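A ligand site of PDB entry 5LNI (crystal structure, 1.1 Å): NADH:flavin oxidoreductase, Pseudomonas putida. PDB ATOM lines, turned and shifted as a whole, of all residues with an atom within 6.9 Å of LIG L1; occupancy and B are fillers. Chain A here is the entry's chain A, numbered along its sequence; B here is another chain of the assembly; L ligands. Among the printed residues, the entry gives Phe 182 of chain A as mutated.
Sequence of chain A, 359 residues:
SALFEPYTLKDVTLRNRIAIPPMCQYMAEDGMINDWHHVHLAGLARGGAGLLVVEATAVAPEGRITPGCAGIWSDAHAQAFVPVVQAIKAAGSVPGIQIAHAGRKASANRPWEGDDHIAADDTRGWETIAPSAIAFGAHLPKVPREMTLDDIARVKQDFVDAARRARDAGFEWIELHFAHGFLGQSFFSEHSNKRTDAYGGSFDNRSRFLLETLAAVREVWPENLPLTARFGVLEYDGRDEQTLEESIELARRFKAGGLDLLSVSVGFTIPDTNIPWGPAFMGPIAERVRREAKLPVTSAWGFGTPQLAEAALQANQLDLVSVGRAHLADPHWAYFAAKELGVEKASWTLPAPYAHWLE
NH2 of Arg 230 sits at hydrogen-bond distance from O1 of LG2 L2 (2.8 Å).
The backbone NH of Cys 24 lies within hydrogen-bond range of a nitrogen (N3) of LG2 L2 (2.9 Å).
An oxygen (O6) of LG2 L2 is in hydrogen-bond range of the backbone NH (N) of Trp 301 (3.1 Å).
An oxygen (O3) of LG2 L2 is in hydrogen-bond range of the backbone carbonyl oxygen of Pro 22 (2.9 Å).
N of Arg 325 lies within hydrogen-bond range of O7 of LG2 L2 (2.8 Å).
NE2 of His 177 sits at hydrogen-bond distance from O1 of LG2 L2 (3.3 Å).
An oxygen (O8) of LG2 L2 lies within salt-bridge range of the guanidinium group (NH2) of Arg 325 (2.9 Å).
An oxygen (O3) of LIG L1 sits at hydrogen-bond distance from a ring nitrogen (NE2) of His 177 (2.8 Å).
An oxygen (O2) of LG2 L2 lies within hydrogen-bond range of the backbone NH (N) of Ala 56 (2.9 Å).
SG of Cys 24 is in hydrogen-bond range of O2 of LG2 L2.
A ring nitrogen (ND1) of His 180 lies within hydrogen-bond range of an oxygen (O3) of LIG L1.
An oxygen (O1) of LG2 L2 sits at hydrogen-bond distance from the side-chain amide nitrogen (NE2) of Gln 98.
An oxygen (O3) of LIG L1 sits close to a nitrogen (N2) of LG2 L2, 3.3 Å away.
ND1 of His 177 sits at hydrogen-bond distance from N of Ala 179 (3.3 Å).
Merely in contact with LIG L1: Tyr 26 (3.4 Å), Ile 65 (3.8 Å), Phe 182 (3.2 Å), Trp 301 (3.6 Å) and Trp 357 of chain B (3.7 Å).
Hydrophobic or aromatic side chains that line LIG L1: Ile 65, His 177, His 180, Phe 182, Trp 301 and Trp 357 of chain B.
Of the 18 residues printed, 7 come within 4 Å of LIG L1.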
ATOM      1  N   PRO A  22       6.694  26.865 -11.371  1.00  0.00           N
ATOM      2  CA  PRO A  22       6.018  26.628 -12.638  1.00  0.00           C
ATOM      3  C   PRO A  22       5.891  25.137 -12.887  1.00  0.00           C
ATOM      4  O   PRO A  22       6.833  24.378 -12.768  1.00  0.00           O
ATOM      5  CB  PRO A  22       6.946  27.304 -13.677  1.00  0.00           C
ATOM      6  CG  PRO A  22       8.296  27.383 -12.975  1.00  0.00           C
ATOM      7  CD  PRO A  22       7.962  27.613 -11.544  1.00  0.00           C
ATOM      8  N   MET A  23       4.687  24.737 -13.288  1.00  0.00           N
ATOM      9  CA  MET A  23       4.381  23.341 -13.636  1.00  0.00           C
ATOM     10  C   MET A  23       3.497  23.267 -14.879  1.00  0.00           C
ATOM     11  O   MET A  23       2.272  23.471 -14.805  1.00  0.00           O
ATOM     12  CB  MET A  23       3.757  22.548 -12.493  1.00  0.00           C
ATOM     13  CG  MET A  23       4.739  22.249 -11.383  1.00  0.00           C
ATOM     14  SD  MET A  23       4.019  21.284 -10.037  1.00  0.00           S
ATOM     15  CE  MET A  23       3.011  22.535  -9.295  1.00  0.00           C
ATOM     16  N   CYS A  24       4.109  23.001 -16.025  1.00  0.00           N
ATOM     17  CA  CYS A  24       3.379  22.768 -17.257  1.00  0.00           C
ATOM     18  C   CYS A  24       2.207  21.821 -17.071  1.00  0.00           C
ATOM     19  O   CYS A  24       2.313  20.761 -16.433  1.00  0.00           O
ATOM     20  CB  CYS A  24       4.313  22.201 -18.297  1.00  0.00           C
ATOM     21  SG  CYS A  24       5.431  23.364 -19.087  1.00  0.00           S
ATOM     22  N   TYR A  26       0.147  21.225 -20.064  1.00  0.00           N
ATOM     23  CA  TYR A  26      -0.040  20.608 -21.388  1.00  0.00           C
ATOM     24  C   TYR A  26      -1.486  20.627 -21.851  1.00  0.00           C
ATOM     25  O   TYR A  26      -1.911  19.738 -22.588  1.00  0.00           O
ATOM     26  CB  TYR A  26       0.586  19.189 -21.447  1.00  0.00           C
ATOM     27  CG  TYR A  26       1.984  19.133 -20.898  1.00  0.00           C
ATOM     28  CD1 TYR A  26       3.087  19.370 -21.701  1.00  0.00           C
ATOM     29  CD2 TYR A  26       2.196  18.844 -19.550  1.00  0.00           C
ATOM     30  CE1 TYR A  26       4.374  19.338 -21.195  1.00  0.00           C
ATOM     31  CE2 TYR A  26       3.479  18.802 -19.036  1.00  0.00           C
ATOM     32  CZ  TYR A  26       4.565  19.023 -19.857  1.00  0.00           C
ATOM     33  OH  TYR A  26       5.823  18.974 -19.304  1.00  0.00           O
ATOM     34  N   ALA A  56       5.778  27.349 -17.539  1.00  0.00           N
ATOM     35  CA  ALA A  56       6.536  27.815 -18.707  1.00  0.00           C
ATOM     36  C   ALA A  56       5.583  28.256 -19.810  1.00  0.00           C
ATOM     37  O   ALA A  56       4.847  27.445 -20.371  1.00  0.00           O
ATOM     38  CB  ALA A  56       7.426  26.698 -19.222  1.00  0.00           C
ATOM     39  N   ILE A  65       7.301  23.730 -25.497  1.00  0.00           N
ATOM     40  CA  ILE A  65       7.819  22.377 -25.429  1.00  0.00           C
ATOM     41  C   ILE A  65       6.952  21.464 -26.312  1.00  0.00           C
ATOM     42  O   ILE A  65       7.483  20.643 -27.050  1.00  0.00           O
ATOM     43  CB  ILE A  65       7.873  21.834 -23.975  1.00  0.00           C
ATOM     44  CG1 ILE A  65       8.578  22.811 -23.035  1.00  0.00           C
ATOM     45  CG2 ILE A  65       8.539  20.465 -23.969  1.00  0.00           C
ATOM     46  CD1 ILE A  65       8.307  22.521 -21.565  1.00  0.00           C
ATOM     47  N   GLN A  98       6.396  32.274 -15.499  1.00  0.00           N
ATOM     48  CA  GLN A  98       7.667  31.896 -16.118  1.00  0.00           C
ATOM     49  C   GLN A  98       7.550  32.026 -17.625  1.00  0.00           C
ATOM     50  O   GLN A  98       6.690  31.375 -18.216  1.00  0.00           O
ATOM     51  CB  GLN A  98       8.043  30.470 -15.730  1.00  0.00           C
ATOM     52  CG  GLN A  98       9.415  30.097 -16.197  1.00  0.00           C
ATOM     53  CD  GLN A  98       9.702  28.643 -16.046  1.00  0.00           C
ATOM     54  OE1 GLN A  98       8.994  27.822 -16.603  1.00  0.00           O
ATOM     55  NE2 GLN A  98      10.750  28.315 -15.287  1.00  0.00           N
ATOM     56  N   PRO A 111       3.952  14.556 -22.079  1.00  0.00           N
ATOM     57  CA  PRO A 111       4.656  13.485 -21.364  1.00  0.00           C
ATOM     58  C   PRO A 111       3.889  12.155 -21.274  1.00  0.00           C
ATOM     59  O   PRO A 111       4.545  11.108 -21.267  1.00  0.00           O
ATOM     60  CB  PRO A 111       4.896  14.103 -19.983  1.00  0.00           C
ATOM     61  CG  PRO A 111       5.027  15.583 -20.298  1.00  0.00           C
ATOM     62  CD  PRO A 111       3.974  15.825 -21.326  1.00  0.00           C
ATOM     63  N   HIS A 177      13.024  31.716 -17.952  1.00  0.00           N
ATOM     64  CA  HIS A 177      13.355  30.299 -17.915  1.00  0.00           C
ATOM     65  C   HIS A 177      14.680  30.073 -18.637  1.00  0.00           C
ATOM     66  O   HIS A 177      14.710  29.794 -19.833  1.00  0.00           O
ATOM     67  CB  HIS A 177      12.249  29.474 -18.554  1.00  0.00           C
ATOM     68  CG  HIS A 177      12.360  28.033 -18.237  1.00  0.00           C
ATOM     69  ND1 HIS A 177      13.467  27.494 -17.602  1.00  0.00           N
ATOM     70  CD2 HIS A 177      11.448  27.028 -18.356  1.00  0.00           C
ATOM     71  CE1 HIS A 177      13.218  26.219 -17.355  1.00  0.00           C
ATOM     72  NE2 HIS A 177      12.007  25.905 -17.806  1.00  0.00           N
ATOM     73  N   ALA A 179      16.733  27.614 -17.600  1.00  0.00           N
ATOM     74  CA  ALA A 179      17.121  26.314 -17.059  1.00  0.00           C
ATOM     75  C   ALA A 179      16.674  25.143 -17.951  1.00  0.00           C
ATOM     76  O   ALA A 179      16.058  25.326 -19.007  1.00  0.00           O
ATOM     77  CB  ALA A 179      16.572  26.153 -15.626  1.00  0.00           C
ATOM     78  N   HIS A 180      17.024  23.948 -17.528  1.00  0.00           N
ATOM     79  CA  HIS A 180      16.391  22.690 -17.979  1.00  0.00           C
ATOM     80  C   HIS A 180      16.664  22.358 -19.421  1.00  0.00           C
ATOM     81  O   HIS A 180      15.903  21.633 -20.066  1.00  0.00           O
ATOM     82  CB  HIS A 180      14.901  22.672 -17.629  1.00  0.00           C
ATOM     83  CG  HIS A 180      14.656  22.874 -16.159  1.00  0.00           C
ATOM     84  ND1 HIS A 180      13.434  23.235 -15.646  1.00  0.00           N
ATOM     85  CD2 HIS A 180      15.499  22.824 -15.093  1.00  0.00           C
ATOM     86  CE1 HIS A 180      13.526  23.381 -14.335  1.00  0.00           C
ATOM     87  NE2 HIS A 180      14.764  23.122 -13.974  1.00  0.00           N
ATOM     88  N   PHE A 182      16.684  24.120 -22.046  1.00  0.00           N
ATOM     89  CA  PHE A 182      15.928  24.897 -23.012  1.00  0.00           C
ATOM     90  C   PHE A 182      16.837  25.996 -23.594  1.00  0.00           C
ATOM     91  O   PHE A 182      18.062  25.917 -23.449  1.00  0.00           O
ATOM     92  CB  PHE A 182      14.664  25.404 -22.340  1.00  0.00           C
ATOM     93  CG  PHE A 182      13.711  24.305 -21.909  1.00  0.00           C
ATOM     94  CD1 PHE A 182      13.329  23.284 -22.748  1.00  0.00           C
ATOM     95  CD2 PHE A 182      13.179  24.327 -20.632  1.00  0.00           C
ATOM     96  CE1 PHE A 182      12.432  22.328 -22.356  1.00  0.00           C
ATOM     97  CE2 PHE A 182      12.277  23.383 -20.226  1.00  0.00           C
ATOM     98  CZ  PHE A 182      11.891  22.368 -21.072  1.00  0.00           C
ATOM     99  N   ARG A 230      15.199  31.323 -13.532  1.00  0.00           N
ATOM    100  CA  ARG A 230      15.543  29.939 -13.205  1.00  0.00           C
ATOM    101  C   ARG A 230      16.761  29.543 -14.030  1.00  0.00           C
ATOM    102  O   ARG A 230      16.807  29.815 -15.227  1.00  0.00           O
ATOM    103  CB  ARG A 230      14.385  28.980 -13.442  1.00  0.00           C
ATOM    104  CG  ARG A 230      14.552  27.659 -12.692  1.00  0.00           C
ATOM    105  CD  ARG A 230      13.270  26.838 -12.652  1.00  0.00           C
ATOM    106  NE  ARG A 230      13.281  25.951 -11.484  1.00  0.00           N
ATOM    107  CZ  ARG A 230      12.292  25.133 -11.147  1.00  0.00           C
ATOM    108  NH1 ARG A 230      12.360  24.483  -9.979  1.00  0.00           N
ATOM    109  NH2 ARG A 230      11.265  24.938 -11.933  1.00  0.00           N
ATOM    110  N   PHE A 268      19.894  19.807 -16.970  1.00  0.00           N
ATOM    111  CA  PHE A 268      19.232  18.900 -17.917  1.00  0.00           C
ATOM    112  C   PHE A 268      19.618  19.194 -19.367  1.00  0.00           C
ATOM    113  O   PHE A 268      18.805  19.036 -20.268  1.00  0.00           O
ATOM    114  CB  PHE A 268      17.702  18.953 -17.820  1.00  0.00           C
ATOM    115  CG  PHE A 268      17.138  18.785 -16.428  1.00  0.00           C
ATOM    116  CD1 PHE A 268      17.735  17.958 -15.483  1.00  0.00           C
ATOM    117  CD2 PHE A 268      15.995  19.474 -16.069  1.00  0.00           C
ATOM    118  CE1 PHE A 268      17.179  17.832 -14.207  1.00  0.00           C
ATOM    119  CE2 PHE A 268      15.452  19.363 -14.802  1.00  0.00           C
ATOM    120  CZ  PHE A 268      16.039  18.531 -13.870  1.00  0.00           C
ATOM    121  N   TRP A 277      19.151  12.282  -7.245  1.00  0.00           N
ATOM    122  CA  TRP A 277      17.824  12.588  -6.717  1.00  0.00           C
ATOM    123  C   TRP A 277      17.674  12.099  -5.295  1.00  0.00           C
ATOM    124  O   TRP A 277      18.054  10.966  -4.985  1.00  0.00           O
ATOM    125  CB  TRP A 277      16.755  11.919  -7.551  1.00  0.00           C
ATOM    126  CG  TRP A 277      16.809  12.239  -8.993  1.00  0.00           C
ATOM    127  CD1 TRP A 277      17.218  11.422 -10.006  1.00  0.00           C
ATOM    128  CD2 TRP A 277      16.440  13.480  -9.613  1.00  0.00           C
ATOM    129  NE1 TRP A 277      17.141  12.077 -11.210  1.00  0.00           N
ATOM    130  CE2 TRP A 277      16.655  13.338 -10.995  1.00  0.00           C
ATOM    131  CE3 TRP A 277      15.963  14.693  -9.120  1.00  0.00           C
ATOM    132  CZ2 TRP A 277      16.394  14.362 -11.896  1.00  0.00           C
ATOM    133  CZ3 TRP A 277      15.700  15.699 -10.021  1.00  0.00           C
ATOM    134  CH2 TRP A 277      15.921  15.528 -11.388  1.00  0.00           C
ATOM    135  N   TRP A 301      12.821  20.126  -6.246  1.00  0.00           N
ATOM    136  CA  TRP A 301      13.312  18.775  -6.516  1.00  0.00           C
ATOM    137  C   TRP A 301      13.570  18.042  -5.214  1.00  0.00           C
ATOM    138  O   TRP A 301      14.640  17.449  -5.023  1.00  0.00           O
ATOM    139  CB  TRP A 301      14.556  18.763  -7.411  1.00  0.00           C
ATOM    140  CG  TRP A 301      14.461  19.594  -8.651  1.00  0.00           C
ATOM    141  CD1 TRP A 301      15.017  20.818  -8.853  1.00  0.00           C
ATOM    142  CD2 TRP A 301      13.771  19.268  -9.872  1.00  0.00           C
ATOM    143  NE1 TRP A 301      14.731  21.271 -10.110  1.00  0.00           N
ATOM    144  CE2 TRP A 301      13.948  20.351 -10.755  1.00  0.00           C
ATOM    145  CE3 TRP A 301      13.002  18.169 -10.286  1.00  0.00           C
ATOM    146  CZ2 TRP A 301      13.396  20.372 -12.044  1.00  0.00           C
ATOM    147  CZ3 TRP A 301      12.473  18.193 -11.557  1.00  0.00           C
ATOM    148  CH2 TRP A 301      12.670  19.286 -12.429  1.00  0.00           C
ATOM    149  N   ARG A 325       5.188  18.899  -6.979  1.00  0.00           N
ATOM    150  CA  ARG A 325       4.311  17.722  -7.084  1.00  0.00           C
ATOM    151  C   ARG A 325       3.371  17.560  -5.913  1.00  0.00           C
ATOM    152  O   ARG A 325       2.251  17.041  -6.086  1.00  0.00           O
ATOM    153  CB  ARG A 325       5.141  16.447  -7.259  1.00  0.00           C
ATOM    154  CG  ARG A 325       5.727  16.291  -8.648  1.00  0.00           C
ATOM    155  CD  ARG A 325       6.762  15.180  -8.697  1.00  0.00           C
ATOM    156  NE  ARG A 325       7.888  15.493  -7.820  1.00  0.00           N
ATOM    157  CZ  ARG A 325       8.509  14.623  -7.020  1.00  0.00           C
ATOM    158  NH1 ARG A 325       8.129  13.352  -6.955  1.00  0.00           N
ATOM    159  NH2 ARG A 325       9.516  15.039  -6.273  1.00  0.00           N
ATOM    160  N   TRP B 357       2.335  12.463 -13.152  1.00  0.00           N
ATOM    161  CA  TRP B 357       3.488  12.817 -12.329  1.00  0.00           C
ATOM    162  C   TRP B 357       3.448  12.166 -10.975  1.00  0.00           C
ATOM    163  O   TRP B 357       4.446  12.198 -10.274  1.00  0.00           O
ATOM    164  CB  TRP B 357       3.524  14.328 -12.169  1.00  0.00           C
ATOM    165  CG  TRP B 357       3.443  14.979 -13.493  1.00  0.00           C
ATOM    166  CD1 TRP B 357       2.363  15.630 -14.012  1.00  0.00           C
ATOM    167  CD2 TRP B 357       4.443  14.965 -14.504  1.00  0.00           C
ATOM    168  NE1 TRP B 357       2.634  16.015 -15.292  1.00  0.00           N
ATOM    169  CE2 TRP B 357       3.904  15.638 -15.610  1.00  0.00           C
ATOM    170  CE3 TRP B 357       5.747  14.459 -14.589  1.00  0.00           C
ATOM    171  CZ2 TRP B 357       4.628  15.846 -16.768  1.00  0.00           C
ATOM    172  CZ3 TRP B 357       6.454  14.658 -15.744  1.00  0.00           C
ATOM    173  CH2 TRP B 357       5.888  15.364 -16.833  1.00  0.00           C
HETATM  174  O1  LIG L   1       9.886  17.307 -14.052  1.00  0.00           O
HETATM  175  C1  LIG L   1       9.517  18.052 -14.976  1.00  0.00           C
HETATM  176  C2  LIG L   1       8.404  17.862 -15.793  1.00  0.00           C
HETATM  177  C3  LIG L   1       8.114  18.787 -16.781  1.00  0.00           C
HETATM  178  C4  LIG L   1       8.907  19.904 -16.991  1.00  0.00           C
HETATM  179  O2  LIG L   1      10.309  19.152 -15.185  1.00  0.00           O
HETATM  180  C5  LIG L   1      10.012  20.073 -16.158  1.00  0.00           C
HETATM  181  C6  LIG L   1      10.866  21.176 -16.240  1.00  0.00           C
HETATM  182  C7  LIG L   1      10.579  22.172 -17.181  1.00  0.00           C
HETATM  183  O3  LIG L   1      11.307  23.247 -17.210  1.00  0.00           O
HETATM  184  C8  LIG L   1       9.478  22.014 -18.036  1.00  0.00           C
HETATM  185  C9  LIG L   1       8.667  20.900 -17.930  1.00  0.00           C
HETATM  186  N1  LG2 L   2       9.944  23.599 -14.188  1.00  0.00           N
HETATM  187  C1  LG2 L   2       9.992  24.756 -14.834  1.00  0.00           C
HETATM  188  O1  LG2 L   2      10.981  25.542 -14.663  1.00  0.00           O
HETATM  189  N2  LG2 L   2       8.971  25.104 -15.725  1.00  0.00           N
HETATM  190  C2  LG2 L   2       7.884  24.388 -15.920  1.00  0.00           C
HETATM  191  O2  LG2 L   2       6.935  24.818 -16.574  1.00  0.00           O
HETATM  192  C3  LG2 L   2       7.874  23.061 -15.318  1.00  0.00           C
HETATM  193  N3  LG2 L   2       6.823  22.215 -15.579  1.00  0.00           N
HETATM  194  C4  LG2 L   2       6.702  21.109 -14.782  1.00  0.00           C
HETATM  195  C5  LG2 L   2       5.519  20.298 -14.883  1.00  0.00           C
HETATM  196  C6  LG2 L   2       5.269  19.289 -13.992  1.00  0.00           C
HETATM  197  C7  LG2 L   2       3.952  18.604 -14.014  1.00  0.00           C
HETATM  198  C8  LG2 L   2       6.260  18.977 -13.019  1.00  0.00           C
HETATM  199  C9  LG2 L   2       6.035  17.839 -12.035  1.00  0.00           C
HETATM  200  C10 LG2 L   2       7.457  19.708 -12.953  1.00  0.00           C
HETATM  201  C11 LG2 L   2       7.660  20.843 -13.791  1.00  0.00           C
HETATM  202  N4  LG2 L   2       8.783  21.652 -13.638  1.00  0.00           N
HETATM  203  C12 LG2 L   2       8.901  22.795 -14.401  1.00  0.00           C
HETATM  204  C13 LG2 L   2       9.691  21.433 -12.499  1.00  0.00           C
HETATM  205  C14 LG2 L   2       9.014  21.889 -11.199  1.00  0.00           C
HETATM  206  O3  LG2 L   2       8.938  23.323 -11.142  1.00  0.00           O
HETATM  207  C15 LG2 L   2       9.780  21.431  -9.949  1.00  0.00           C
HETATM  208  O4  LG2 L   2      11.136  21.861 -10.034  1.00  0.00           O
HETATM  209  C16 LG2 L   2       9.713  19.919  -9.778  1.00  0.00           C
HETATM  210  O5  LG2 L   2       8.353  19.511  -9.715  1.00  0.00           O
HETATM  211  C17 LG2 L   2      10.501  19.481  -8.539  1.00  0.00           C
HETATM  212  O6  LG2 L   2       9.906  19.952  -7.321  1.00  0.00           O
HETATM  213  P1  LG2 L   2       9.032  18.920  -6.417  1.00  0.00           P
HETATM  214  O7  LG2 L   2       7.959  18.365  -7.338  1.00  0.00           O
HETATM  215  O8  LG2 L   2       9.986  17.846  -5.950  1.00  0.00           O
HETATM  216  O9  LG2 L   2       8.495  19.769  -5.308  1.00  0.00           O
